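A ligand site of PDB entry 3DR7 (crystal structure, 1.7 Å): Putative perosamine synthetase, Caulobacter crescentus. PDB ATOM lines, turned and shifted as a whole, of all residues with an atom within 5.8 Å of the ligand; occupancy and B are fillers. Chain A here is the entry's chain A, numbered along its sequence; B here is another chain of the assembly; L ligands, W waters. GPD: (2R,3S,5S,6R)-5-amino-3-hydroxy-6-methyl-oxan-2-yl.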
ATOM      1  N   THR A  48       9.933   6.831 -18.463  1.00  0.00           N
ATOM      2  CA  THR A  48       9.503   5.535 -17.995  1.00  0.00           C
ATOM      3  C   THR A  48       8.007   5.435 -17.881  1.00  0.00           C
ATOM      4  O   THR A  48       7.539   4.333 -17.642  1.00  0.00           O
ATOM      5  CB  THR A  48      10.147   5.204 -16.676  1.00  0.00           C
ATOM      6  OG1 THR A  48       9.738   6.159 -15.695  1.00  0.00           O
ATOM      7  CG2 THR A  48      11.610   5.417 -16.868  1.00  0.00           C
ATOM      8  N   THR A  49       7.291   6.542 -18.111  1.00  0.00           N
ATOM      9  CA  THR A  49       5.819   6.624 -18.007  1.00  0.00           C
ATOM     10  C   THR A  49       5.242   6.547 -16.582  1.00  0.00           C
ATOM     11  O   THR A  49       4.027   6.548 -16.371  1.00  0.00           O
ATOM     12  CB  THR A  49       5.110   5.634 -18.947  1.00  0.00           C
ATOM     13  OG1 THR A  49       5.000   4.386 -18.277  1.00  0.00           O
ATOM     14  CG2 THR A  49       6.001   5.413 -20.109  1.00  0.00           C
ATOM     15  N   TRP A  50       6.114   6.558 -15.587  1.00  0.00           N
ATOM     16  CA  TRP A  50       5.629   6.586 -14.233  1.00  0.00           C
ATOM     17  C   TRP A  50       5.567   8.047 -13.765  1.00  0.00           C
ATOM     18  O   TRP A  50       6.520   8.600 -13.251  1.00  0.00           O
ATOM     19  CB  TRP A  50       6.611   5.762 -13.350  1.00  0.00           C
ATOM     20  CG  TRP A  50       6.496   4.325 -13.707  1.00  0.00           C
ATOM     21  CD1 TRP A  50       7.395   3.604 -14.429  1.00  0.00           C
ATOM     22  CD2 TRP A  50       5.344   3.470 -13.544  1.00  0.00           C
ATOM     23  NE1 TRP A  50       6.908   2.352 -14.696  1.00  0.00           N
ATOM     24  CE2 TRP A  50       5.615   2.272 -14.238  1.00  0.00           C
ATOM     25  CE3 TRP A  50       4.071   3.634 -12.975  1.00  0.00           C
ATOM     26  CZ2 TRP A  50       4.672   1.224 -14.346  1.00  0.00           C
ATOM     27  CZ3 TRP A  50       3.135   2.579 -13.054  1.00  0.00           C
ATOM     28  CH2 TRP A  50       3.458   1.388 -13.709  1.00  0.00           C
ATOM     29  N   ILE A  51       4.412   8.666 -13.924  1.00  0.00           N
ATOM     30  CA  ILE A  51       4.221  10.064 -13.556  1.00  0.00           C
ATOM     31  C   ILE A  51       3.176  10.279 -12.439  1.00  0.00           C
ATOM     32  O   ILE A  51       3.034  11.390 -11.891  1.00  0.00           O
ATOM     33  CB  ILE A  51       3.891  10.888 -14.847  1.00  0.00           C
ATOM     34  CG1 ILE A  51       2.669  10.315 -15.549  1.00  0.00           C
ATOM     35  CG2 ILE A  51       5.093  10.833 -15.865  1.00  0.00           C
ATOM     36  CD1 ILE A  51       1.868  11.318 -16.393  1.00  0.00           C
ATOM     37  N   SER A  52       2.446   9.217 -12.073  1.00  0.00           N
ATOM     38  CA  SER A  52       1.422   9.313 -11.038  1.00  0.00           C
ATOM     39  C   SER A  52       2.015   9.132  -9.634  1.00  0.00           C
ATOM     40  O   SER A  52       3.195   9.336  -9.433  1.00  0.00           O
ATOM     41  CB  SER A  52       0.320   8.286 -11.292  1.00  0.00           C
ATOM     42  OG  SER A  52      -0.908   8.713 -10.760  1.00  0.00           O
ATOM     43  N   SER A  53       1.192   8.702  -8.673  1.00  0.00           N
ATOM     44  CA  SER A  53       1.682   8.486  -7.321  1.00  0.00           C
ATOM     45  C   SER A  53       2.282   7.087  -7.238  1.00  0.00           C
ATOM     46  O   SER A  53       2.588   6.604  -6.139  1.00  0.00           O
ATOM     47  CB  SER A  53       0.534   8.596  -6.326  1.00  0.00           C
ATOM     48  OG  SER A  53      -0.577   7.871  -6.830  1.00  0.00           O
ATOM     49  N   VAL A  54       2.486   6.454  -8.384  1.00  0.00           N
ATOM     50  CA  VAL A  54       3.111   5.118  -8.477  1.00  0.00           C
ATOM     51  C   VAL A  54       4.475   5.370  -9.178  1.00  0.00           C
ATOM     52  O   VAL A  54       4.516   5.903 -10.301  1.00  0.00           O
ATOM     53  CB  VAL A  54       2.239   4.142  -9.354  1.00  0.00           C
ATOM     54  CG1 VAL A  54       2.992   2.884  -9.761  1.00  0.00           C
ATOM     55  CG2 VAL A  54       0.901   3.762  -8.690  1.00  0.00           C
ATOM     56  N   GLN A 233      -5.932   6.756   0.526  1.00  0.00           N
ATOM     57  CA  GLN A 233      -7.377   6.665   0.463  1.00  0.00           C
ATOM     58  C   GLN A 233      -7.868   5.694   1.472  1.00  0.00           C
ATOM     59  O   GLN A 233      -8.986   5.171   1.317  1.00  0.00           O
ATOM     60  CB  GLN A 233      -7.841   6.226  -0.953  1.00  0.00           C
ATOM     61  CG  GLN A 233      -7.512   7.264  -2.107  1.00  0.00           C
ATOM     62  CD  GLN A 233      -8.618   8.338  -2.131  1.00  0.00           C
ATOM     63  OE1 GLN A 233      -9.236   8.596  -1.082  1.00  0.00           O
ATOM     64  NE2 GLN A 233      -8.773   9.025  -3.241  1.00  0.00           N
ATOM     65  N   MET A 235      -7.132   2.635   1.866  1.00  0.00           N
ATOM     66  CA  MET A 235      -7.322   1.298   1.287  1.00  0.00           C
ATOM     67  C   MET A 235      -6.447   0.208   1.869  1.00  0.00           C
ATOM     68  O   MET A 235      -5.259   0.383   2.053  1.00  0.00           O
ATOM     69  CB  MET A 235      -7.171   1.244  -0.243  1.00  0.00           C
ATOM     70  CG  MET A 235      -7.800   0.029  -0.939  1.00  0.00           C
ATOM     71  SD  MET A 235      -7.622   0.102  -2.763  1.00  0.00           S
ATOM     72  CE  MET A 235      -5.903  -0.299  -2.998  1.00  0.00           C
ATOM     73  N   ARG A 240      -7.945  -5.200  -2.717  1.00  0.00           N
ATOM     74  CA  ARG A 240      -8.342  -4.206  -3.721  1.00  0.00           C
ATOM     75  C   ARG A 240      -9.678  -3.549  -3.457  1.00  0.00           C
ATOM     76  O   ARG A 240     -10.706  -4.208  -3.377  1.00  0.00           O
ATOM     77  CB  ARG A 240      -8.349  -4.745  -5.163  1.00  0.00           C
ATOM     78  CG  ARG A 240      -8.287  -3.671  -6.285  1.00  0.00           C
ATOM     79  CD  ARG A 240      -7.042  -2.784  -6.286  1.00  0.00           C
ATOM     80  NE  ARG A 240      -5.797  -3.545  -6.479  1.00  0.00           N
ATOM     81  CZ  ARG A 240      -4.576  -2.994  -6.483  1.00  0.00           C
ATOM     82  NH1 ARG A 240      -4.402  -1.680  -6.294  1.00  0.00           N
ATOM     83  NH2 ARG A 240      -3.507  -3.759  -6.663  1.00  0.00           N
ATOM     84  N   TYR A 241      -9.641  -2.226  -3.380  1.00  0.00           N
ATOM     85  CA  TYR A 241     -10.899  -1.527  -3.193  1.00  0.00           C
ATOM     86  C   TYR A 241     -11.627  -1.956  -1.933  1.00  0.00           C
ATOM     87  O   TYR A 241     -12.859  -1.784  -1.894  1.00  0.00           O
ATOM     88  CB  TYR A 241     -11.865  -1.686  -4.376  1.00  0.00           C
ATOM     89  CG  TYR A 241     -11.313  -1.191  -5.710  1.00  0.00           C
ATOM     90  CD1 TYR A 241     -10.233  -0.299  -5.755  1.00  0.00           C
ATOM     91  CD2 TYR A 241     -11.801  -1.703  -6.929  1.00  0.00           C
ATOM     92  CE1 TYR A 241      -9.656   0.069  -6.969  1.00  0.00           C
ATOM     93  CE2 TYR A 241     -11.289  -1.298  -8.158  1.00  0.00           C
ATOM     94  CZ  TYR A 241     -10.214  -0.394  -8.177  1.00  0.00           C
ATOM     95  OH  TYR A 241      -9.651  -0.017  -9.414  1.00  0.00           O
ATOM     96  N   SER B  28      -1.059  -4.862 -18.067  1.00  0.00           N
ATOM     97  CA  SER B  28      -1.647  -4.005 -17.036  1.00  0.00           C
ATOM     98  C   SER B  28      -3.095  -3.682 -17.313  1.00  0.00           C
ATOM     99  O   SER B  28      -3.520  -3.628 -18.494  1.00  0.00           O
ATOM    100  CB  SER B  28      -0.877  -2.718 -16.847  1.00  0.00           C
ATOM    101  OG  SER B  28       0.439  -3.038 -16.407  1.00  0.00           O
ATOM    102  N   VAL B  29      -3.842  -3.484 -16.222  1.00  0.00           N
ATOM    103  CA  VAL B  29      -5.251  -3.183 -16.401  1.00  0.00           C
ATOM    104  C   VAL B  29      -5.401  -1.779 -17.007  1.00  0.00           C
ATOM    105  O   VAL B  29      -6.377  -1.444 -17.671  1.00  0.00           O
ATOM    106  CB  VAL B  29      -6.030  -3.400 -15.110  1.00  0.00           C
ATOM    107  CG1 VAL B  29      -5.678  -2.319 -14.088  1.00  0.00           C
ATOM    108  CG2 VAL B  29      -7.519  -3.416 -15.433  1.00  0.00           C
ATOM    109  N   ALA B  30      -4.394  -0.943 -16.825  1.00  0.00           N
ATOM    110  CA  ALA B  30      -4.452   0.404 -17.354  1.00  0.00           C
ATOM    111  C   ALA B  30      -3.048   1.022 -17.448  1.00  0.00           C
ATOM    112  O   ALA B  30      -2.070   0.533 -16.885  1.00  0.00           O
ATOM    113  CB  ALA B  30      -5.340   1.237 -16.396  1.00  0.00           C
ATOM    114  N   ALA B  31      -2.932   2.114 -18.178  1.00  0.00           N
ATOM    115  CA  ALA B  31      -1.657   2.812 -18.336  1.00  0.00           C
ATOM    116  C   ALA B  31      -1.918   3.950 -19.285  1.00  0.00           C
ATOM    117  O   ALA B  31      -2.700   3.813 -20.226  1.00  0.00           O
ATOM    118  CB  ALA B  31      -0.600   1.881 -18.989  1.00  0.00           C
ATOM    119  N   PRO B  32      -1.195   5.036 -19.026  1.00  0.00           N
ATOM    120  CA  PRO B  32      -1.297   6.283 -19.755  1.00  0.00           C
ATOM    121  C   PRO B  32      -0.454   6.128 -21.038  1.00  0.00           C
ATOM    122  O   PRO B  32       0.503   5.352 -21.092  1.00  0.00           O
ATOM    123  CB  PRO B  32      -0.640   7.288 -18.769  1.00  0.00           C
ATOM    124  CG  PRO B  32       0.340   6.495 -18.021  1.00  0.00           C
ATOM    125  CD  PRO B  32      -0.408   5.196 -17.801  1.00  0.00           C
ATOM    126  N   TYR B 106     -16.637   4.542  -6.526  1.00  0.00           N
ATOM    127  CA  TYR B 106     -15.310   4.607  -5.918  1.00  0.00           C
ATOM    128  C   TYR B 106     -15.521   5.396  -4.624  1.00  0.00           C
ATOM    129  O   TYR B 106     -16.319   6.347  -4.597  1.00  0.00           O
ATOM    130  CB  TYR B 106     -14.313   5.251  -6.857  1.00  0.00           C
ATOM    131  CG  TYR B 106     -12.985   5.293  -6.205  1.00  0.00           C
ATOM    132  CD1 TYR B 106     -12.230   4.131  -6.029  1.00  0.00           C
ATOM    133  CD2 TYR B 106     -12.510   6.500  -5.712  1.00  0.00           C
ATOM    134  CE1 TYR B 106     -11.023   4.170  -5.408  1.00  0.00           C
ATOM    135  CE2 TYR B 106     -11.294   6.566  -5.087  1.00  0.00           C
ATOM    136  CZ  TYR B 106     -10.572   5.393  -4.920  1.00  0.00           C
ATOM    137  OH  TYR B 106      -9.325   5.448  -4.370  1.00  0.00           O
ATOM    138  N   GLU B 180     -14.559   9.003 -14.458  1.00  0.00           N
ATOM    139  CA  GLU B 180     -14.275   7.876 -15.327  1.00  0.00           C
ATOM    140  C   GLU B 180     -14.885   8.089 -16.711  1.00  0.00           C
ATOM    141  O   GLU B 180     -14.969   7.184 -17.531  1.00  0.00           O
ATOM    142  CB  GLU B 180     -14.874   6.615 -14.688  1.00  0.00           C
ATOM    143  CG  GLU B 180     -14.104   6.136 -13.503  1.00  0.00           C
ATOM    144  CD  GLU B 180     -14.856   5.067 -12.724  1.00  0.00           C
ATOM    145  OE1 GLU B 180     -15.612   4.271 -13.337  1.00  0.00           O
ATOM    146  OE2 GLU B 180     -14.594   4.999 -11.490  1.00  0.00           O
ATOM    147  N   PHE B 203      -5.918  10.847 -12.477  1.00  0.00           N
ATOM    148  CA  PHE B 203      -4.977   9.847 -11.964  1.00  0.00           C
ATOM    149  C   PHE B 203      -4.458   9.079 -13.173  1.00  0.00           C
ATOM    150  O   PHE B 203      -5.078   9.071 -14.229  1.00  0.00           O
ATOM    151  CB  PHE B 203      -5.689   8.876 -11.009  1.00  0.00           C
ATOM    152  CG  PHE B 203      -4.757   7.865 -10.382  1.00  0.00           C
ATOM    153  CD1 PHE B 203      -3.566   8.233  -9.691  1.00  0.00           C
ATOM    154  CD2 PHE B 203      -5.020   6.493 -10.561  1.00  0.00           C
ATOM    155  CE1 PHE B 203      -2.692   7.239  -9.187  1.00  0.00           C
ATOM    156  CE2 PHE B 203      -4.101   5.505 -10.083  1.00  0.00           C
ATOM    157  CZ  PHE B 203      -2.934   5.895  -9.431  1.00  0.00           C
ATOM    158  N   GLY B 204      -3.346   8.385 -12.987  1.00  0.00           N
ATOM    159  CA  GLY B 204      -2.617   7.643 -14.021  1.00  0.00           C
ATOM    160  C   GLY B 204      -3.324   6.550 -14.807  1.00  0.00           C
ATOM    161  O   GLY B 204      -2.868   6.204 -15.927  1.00  0.00           O
ATOM    162  N   ASN B 205      -4.408   5.993 -14.246  1.00  0.00           N
ATOM    163  CA  ASN B 205      -5.192   4.958 -14.980  1.00  0.00           C
ATOM    164  C   ASN B 205      -6.368   5.574 -15.756  1.00  0.00           C
ATOM    165  O   ASN B 205      -7.128   4.850 -16.427  1.00  0.00           O
ATOM    166  CB  ASN B 205      -5.745   3.863 -14.013  1.00  0.00           C
ATOM    167  CG  ASN B 205      -6.705   4.404 -12.978  1.00  0.00           C
ATOM    168  OD1 ASN B 205      -6.964   5.619 -12.895  1.00  0.00           O
ATOM    169  ND2 ASN B 205      -7.206   3.521 -12.149  1.00  0.00           N
ATOM    170  N1  LLP B 206     -14.550   8.994  -8.178  1.00  0.00           N
ATOM    171  C2  LLP B 206     -14.513   8.122  -9.132  1.00  0.00           C
ATOM    172  C2' LLP B 206     -15.827   7.572  -9.690  1.00  0.00           C
ATOM    173  C3  LLP B 206     -13.292   7.727  -9.665  1.00  0.00           C
ATOM    174  O3  LLP B 206     -13.239   6.847 -10.684  1.00  0.00           O
ATOM    175  C4  LLP B 206     -12.089   8.230  -9.203  1.00  0.00           C
ATOM    176  C4' LLP B 206     -10.806   7.828  -9.839  1.00  0.00           C
ATOM    177  C5  LLP B 206     -12.175   9.173  -8.141  1.00  0.00           C
ATOM    178  C6  LLP B 206     -13.432   9.501  -7.680  1.00  0.00           C
ATOM    179  C5' LLP B 206     -10.970   9.761  -7.449  1.00  0.00           C
ATOM    180  OP4 LLP B 206     -10.190  10.711  -8.158  1.00  0.00           O
ATOM    181  P   LLP B 206      -8.635  10.652  -7.650  1.00  0.00           P
ATOM    182  OP1 LLP B 206      -8.466  11.236  -6.180  1.00  0.00           O
ATOM    183  OP2 LLP B 206      -7.986  11.652  -8.704  1.00  0.00           O
ATOM    184  OP3 LLP B 206      -8.008   9.209  -7.819  1.00  0.00           O
ATOM    185  N   LLP B 206      -6.556   6.889 -15.682  1.00  0.00           N
ATOM    186  CA  LLP B 206      -7.747   7.431 -16.354  1.00  0.00           C
ATOM    187  CB  LLP B 206      -8.368   8.587 -15.552  1.00  0.00           C
ATOM    188  CG  LLP B 206      -8.299   8.506 -14.008  1.00  0.00           C
ATOM    189  CD  LLP B 206      -9.577   7.913 -13.381  1.00  0.00           C
ATOM    190  CE  LLP B 206      -9.472   7.423 -11.914  1.00  0.00           C
ATOM    191  NZ  LLP B 206     -10.726   7.728 -11.122  1.00  0.00           N
ATOM    192  C   LLP B 206      -7.566   7.735 -17.841  1.00  0.00           C
ATOM    193  O   LLP B 206      -6.466   7.694 -18.353  1.00  0.00           O
ATOM    194  N   GLY B 211      -1.015  12.319 -14.117  1.00  0.00           N
ATOM    195  CA  GLY B 211      -0.294  11.667 -13.051  1.00  0.00           C
ATOM    196  C   GLY B 211      -1.268  11.682 -11.816  1.00  0.00           C
ATOM    197  O   GLY B 211      -1.843  10.666 -11.504  1.00  0.00           O
ATOM    198  N   TRP B 306     -13.871   3.678 -20.164  1.00  0.00           N
ATOM    199  CA  TRP B 306     -12.701   3.854 -19.330  1.00  0.00           C
ATOM    200  C   TRP B 306     -12.270   2.408 -19.036  1.00  0.00           C
ATOM    201  O   TRP B 306     -11.064   2.111 -19.044  1.00  0.00           O
ATOM    202  CB  TRP B 306     -13.083   4.554 -18.014  1.00  0.00           C
ATOM    203  CG  TRP B 306     -11.918   4.570 -17.112  1.00  0.00           C
ATOM    204  CD1 TRP B 306     -10.665   4.994 -17.375  1.00  0.00           C
ATOM    205  CD2 TRP B 306     -11.875   4.000 -15.802  1.00  0.00           C
ATOM    206  NE1 TRP B 306      -9.809   4.652 -16.350  1.00  0.00           N
ATOM    207  CE2 TRP B 306     -10.553   4.087 -15.348  1.00  0.00           C
ATOM    208  CE3 TRP B 306     -12.833   3.370 -15.004  1.00  0.00           C
ATOM    209  CZ2 TRP B 306     -10.147   3.588 -14.117  1.00  0.00           C
ATOM    210  CZ3 TRP B 306     -12.421   2.876 -13.766  1.00  0.00           C
ATOM    211  CH2 TRP B 306     -11.096   3.016 -13.322  1.00  0.00           C
ATOM    212  N   GLU B 333      -3.396  -8.385 -15.429  1.00  0.00           N
ATOM    213  CA  GLU B 333      -3.948  -7.576 -14.351  1.00  0.00           C
ATOM    214  C   GLU B 333      -5.435  -7.325 -14.577  1.00  0.00           C
ATOM    215  O   GLU B 333      -5.877  -7.128 -15.696  1.00  0.00           O
ATOM    216  CB  GLU B 333      -3.227  -6.231 -14.319  1.00  0.00           C
ATOM    217  CG  GLU B 333      -3.401  -5.560 -12.978  1.00  0.00           C
ATOM    218  CD  GLU B 333      -2.562  -4.330 -12.835  1.00  0.00           C
ATOM    219  OE1 GLU B 333      -2.481  -3.576 -13.833  1.00  0.00           O
ATOM    220  OE2 GLU B 333      -1.990  -4.137 -11.734  1.00  0.00           O
ATOM    221  N   ARG B 335      -9.339  -5.865 -12.333  1.00  0.00           N
ATOM    222  CA  ARG B 335      -9.875  -5.283 -11.103  1.00  0.00           C
ATOM    223  C   ARG B 335     -11.314  -5.698 -10.913  1.00  0.00           C
ATOM    224  O   ARG B 335     -12.053  -6.049 -11.862  1.00  0.00           O
ATOM    225  CB  ARG B 335      -9.819  -3.738 -11.089  1.00  0.00           C
ATOM    226  CG  ARG B 335      -8.443  -3.070 -11.165  1.00  0.00           C
ATOM    227  CD  ARG B 335      -7.721  -3.055  -9.820  1.00  0.00           C
ATOM    228  NE  ARG B 335      -6.369  -2.465  -9.839  1.00  0.00           N
ATOM    229  CZ  ARG B 335      -5.250  -3.159 -10.034  1.00  0.00           C
ATOM    230  NH1 ARG B 335      -5.309  -4.465 -10.291  1.00  0.00           N
ATOM    231  NH2 ARG B 335      -4.072  -2.539  -9.977  1.00  0.00           N
ATOM    232  N   PHE B 338     -16.254  -2.209  -7.994  1.00  0.00           N
ATOM    233  CA  PHE B 338     -16.150  -1.847  -6.599  1.00  0.00           C
ATOM    234  C   PHE B 338     -16.931  -2.632  -5.524  1.00  0.00           C
ATOM    235  O   PHE B 338     -18.089  -3.021  -5.736  1.00  0.00           O
ATOM    236  CB  PHE B 338     -16.497  -0.378  -6.369  1.00  0.00           C
ATOM    237  CG  PHE B 338     -15.917   0.551  -7.379  1.00  0.00           C
ATOM    238  CD1 PHE B 338     -14.552   0.871  -7.331  1.00  0.00           C
ATOM    239  CD2 PHE B 338     -16.750   1.142  -8.327  1.00  0.00           C
ATOM    240  CE1 PHE B 338     -14.001   1.704  -8.254  1.00  0.00           C
ATOM    241  CE2 PHE B 338     -16.210   2.008  -9.292  1.00  0.00           C
ATOM    242  CZ  PHE B 338     -14.824   2.270  -9.252  1.00  0.00           C
HETATM  243  N4A GPD L   1     -10.610   5.817  -7.929  1.00  0.00           N
HETATM  244  C4G GPD L   1      -9.645   5.257  -8.738  1.00  0.00           C
HETATM  245  C5G GPD L   1      -9.637   3.752  -8.917  1.00  0.00           C
HETATM  246  C6G GPD L   1     -10.878   3.536  -9.827  1.00  0.00           C
HETATM  247  O5G GPD L   1      -8.346   3.650  -9.527  1.00  0.00           O
HETATM  248  C3G GPD L   1      -8.267   5.690  -8.342  1.00  0.00           C
HETATM  249  C2G GPD L   1      -7.455   4.663  -7.636  1.00  0.00           C
HETATM  250  O2G GPD L   1      -6.297   5.409  -7.372  1.00  0.00           O
HETATM  251  C1G GPD L   1      -7.191   3.576  -8.688  1.00  0.00           C
HETATM  252  O1G GPD L   1      -6.925   2.348  -7.958  1.00  0.00           O
HETATM  253  P2  GPD L   1      -6.180   1.261  -8.473  1.00  0.00           P
HETATM  254  O3P GPD L   1      -6.917   0.490  -9.508  1.00  0.00           O
HETATM  255  O4P GPD L   1      -5.773   0.461  -7.361  1.00  0.00           O
HETATM  256  OPP GPD L   1      -4.837   2.005  -9.007  1.00  0.00           O
HETATM  257  P   GPD L   1      -3.387   1.458  -9.276  1.00  0.00           P
HETATM  258  O1P GPD L   1      -3.410   0.150  -8.998  1.00  0.00           O
HETATM  259  O2P GPD L   1      -2.420   2.235  -8.532  1.00  0.00           O
HETATM  260  O5' GPD L   1      -3.155   1.719 -10.820  1.00  0.00           O
HETATM  261  C5' GPD L   1      -4.040   1.182 -11.702  1.00  0.00           C
HETATM  262  C4' GPD L   1      -3.372   0.740 -12.972  1.00  0.00           C
HETATM  263  O4' GPD L   1      -2.837   1.901 -13.608  1.00  0.00           O
HETATM  264  C3' GPD L   1      -2.171  -0.110 -12.724  1.00  0.00           C
HETATM  265  O3' GPD L   1      -1.822  -1.135 -13.597  1.00  0.00           O
HETATM  266  C2' GPD L   1      -1.017   0.819 -12.636  1.00  0.00           C
HETATM  267  O2' GPD L   1       0.233   0.346 -12.822  1.00  0.00           O
HETATM  268  C1' GPD L   1      -1.490   1.977 -13.471  1.00  0.00           C
HETATM  269  N9  GPD L   1      -0.702   3.189 -13.434  1.00  0.00           N
HETATM  270  C8  GPD L   1      -1.068   4.183 -12.613  1.00  0.00           C
HETATM  271  N7  GPD L   1      -0.269   5.200 -12.759  1.00  0.00           N
HETATM  272  C4  GPD L   1       0.226   3.621 -14.206  1.00  0.00           C
HETATM  273  C5  GPD L   1       0.535   4.909 -13.762  1.00  0.00           C
HETATM  274  C6  GPD L   1       1.547   5.724 -14.351  1.00  0.00           C
HETATM  275  O6  GPD L   1       1.814   6.843 -13.978  1.00  0.00           O
HETATM  276  N3  GPD L   1       0.974   3.157 -15.194  1.00  0.00           N
HETATM  277  C2  GPD L   1       1.926   3.873 -15.755  1.00  0.00           C
HETATM  278  N1  GPD L   1       2.242   5.056 -15.363  1.00  0.00           N
HETATM  279  N2  GPD L   1       2.588   3.350 -16.692  1.00  0.00           N
HETATM  280  O   HOH W   1      -7.266   7.877  -5.714  1.00  0.00           O
HETATM  281  O   HOH W   2       1.333  -1.507 -14.285  1.00  0.00           O
HETATM  282  O   HOH W   3       1.141  -0.233 -10.310  1.00  0.00           O
HETATM  283  O   HOH W   4      -3.358   4.026  -6.783  1.00  0.00           O
HETATM  284  O   HOH W   5       0.617   0.534 -16.174  1.00  0.00           O
HETATM  285  O   HOH W   6      -4.463   2.157  -5.264  1.00  0.00           O
HETATM  286  O   HOH W   7      -7.170   0.641 -12.263  1.00  0.00           O
HETATM  287  O   HOH W   8       2.856   0.230 -17.887  1.00  0.00           O
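The guanidinium group (NH1) of Arg 240 lies within salt-bridge range of an oxygen (O4P) of the ligand (2.8 Å).
NH2 of Arg 335 of chain B is in salt-bridge range of O1P of the ligand.
An oxygen (O3P) of the ligand is in hydrogen-bond range of the side-chain hydroxyl (OH) of Tyr 241 (2.8 Å).
The backbone NH (N) of Ile 51 lies within hydrogen-bond range of an oxygen (O6) of the ligand (3.2 Å).
O of Thr 49 sits at hydrogen-bond distance from N1 of the ligand, 2.5 Å away.
OE1 of Glu 333 of chain B lies within hydrogen-bond range of O3' of the ligand, at 2.5 Å.
OG1 of Thr 49 sits at hydrogen-bond distance from N2 of the ligand.
The backbone NH (N) of Ser 52 is in hydrogen-bond range of an oxygen (O6) of the ligand (3.1 Å).
ND2 of Asn 205 of chain B sits at hydrogen-bond distance from O5G of the ligand.
Water W2 lies within hydrogen-bond range of O2' of the ligand (2.6 Å) and OG of Ser 28 of chain B (2.8 Å).
Water W7 lies within hydrogen-bond range of O3P of the ligand and ND2 of Asn 205 of chain B.
Water W5 bridges O of Ala 30 of chain B and N3 of the ligand.
Water W1 lies within hydrogen-bond range of OP3 of LLP 206 of chain B, NE2 of Gln 233, O2G of the ligand and OH of Tyr 106 of chain B.
The side-chain sulfur of Met 235 sits at hydrogen-bond distance from the backbone NH of Tyr 241.
O3 of LLP 206 of chain B sits at hydrogen-bond distance from OE2 of Glu 180 of chain B.
O of Gly 211 of chain B lies within hydrogen-bond range of N of Gly 204 of chain B, at 3.1 Å.
The side-chain carboxylate (OE2) of Glu 333 of chain B is in salt-bridge range of the guanidinium group (NH2) of Arg 335 of chain B (3.2 Å).
OE1 of Glu 333 of chain B sits at hydrogen-bond distance from N of Val 29 of chain B.
OG of Ser 52 lies within hydrogen-bond range of N of Gly 204 of chain B, at 3.3 Å.
The indole nitrogen of Trp 306 of chain B lies within hydrogen-bond range of the backbone carbonyl oxygen of Asn 205 of chain B (2.7 Å).
CZ3 of Trp 50 touches N3 of the ligand, 3.1 Å away.
Val 54 touches the ligand (CG2 to O2P, 3.7 Å).
Ser 28 of chain B touches the ligand (CB to O3', 3.7 Å).
CG1 of Val 29 of chain B touches C4' of the ligand, at 3.99 Å.
Ala 30 of chain B touches the ligand (O to O4', 3.6 Å).
Pro 32 of chain B touches the ligand.
Tyr 106 of chain B touches the ligand (CG to N4A, 3.0 Å).
Phe 203 of chain B touches the ligand.
CA of Gly 204 of chain B touches N7 of the ligand, 3.6 Å away.
C4' of LLP 206 of chain B touches N4A of the ligand, at 2.8 Å.
Trp 306 of chain B touches the ligand.
CE1 of Phe 338 of chain B touches C6G of the ligand, 3.9 Å away.
The nearest printed residue that does not touch the ligand is Ala 31 of chain B (4.1 Å).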
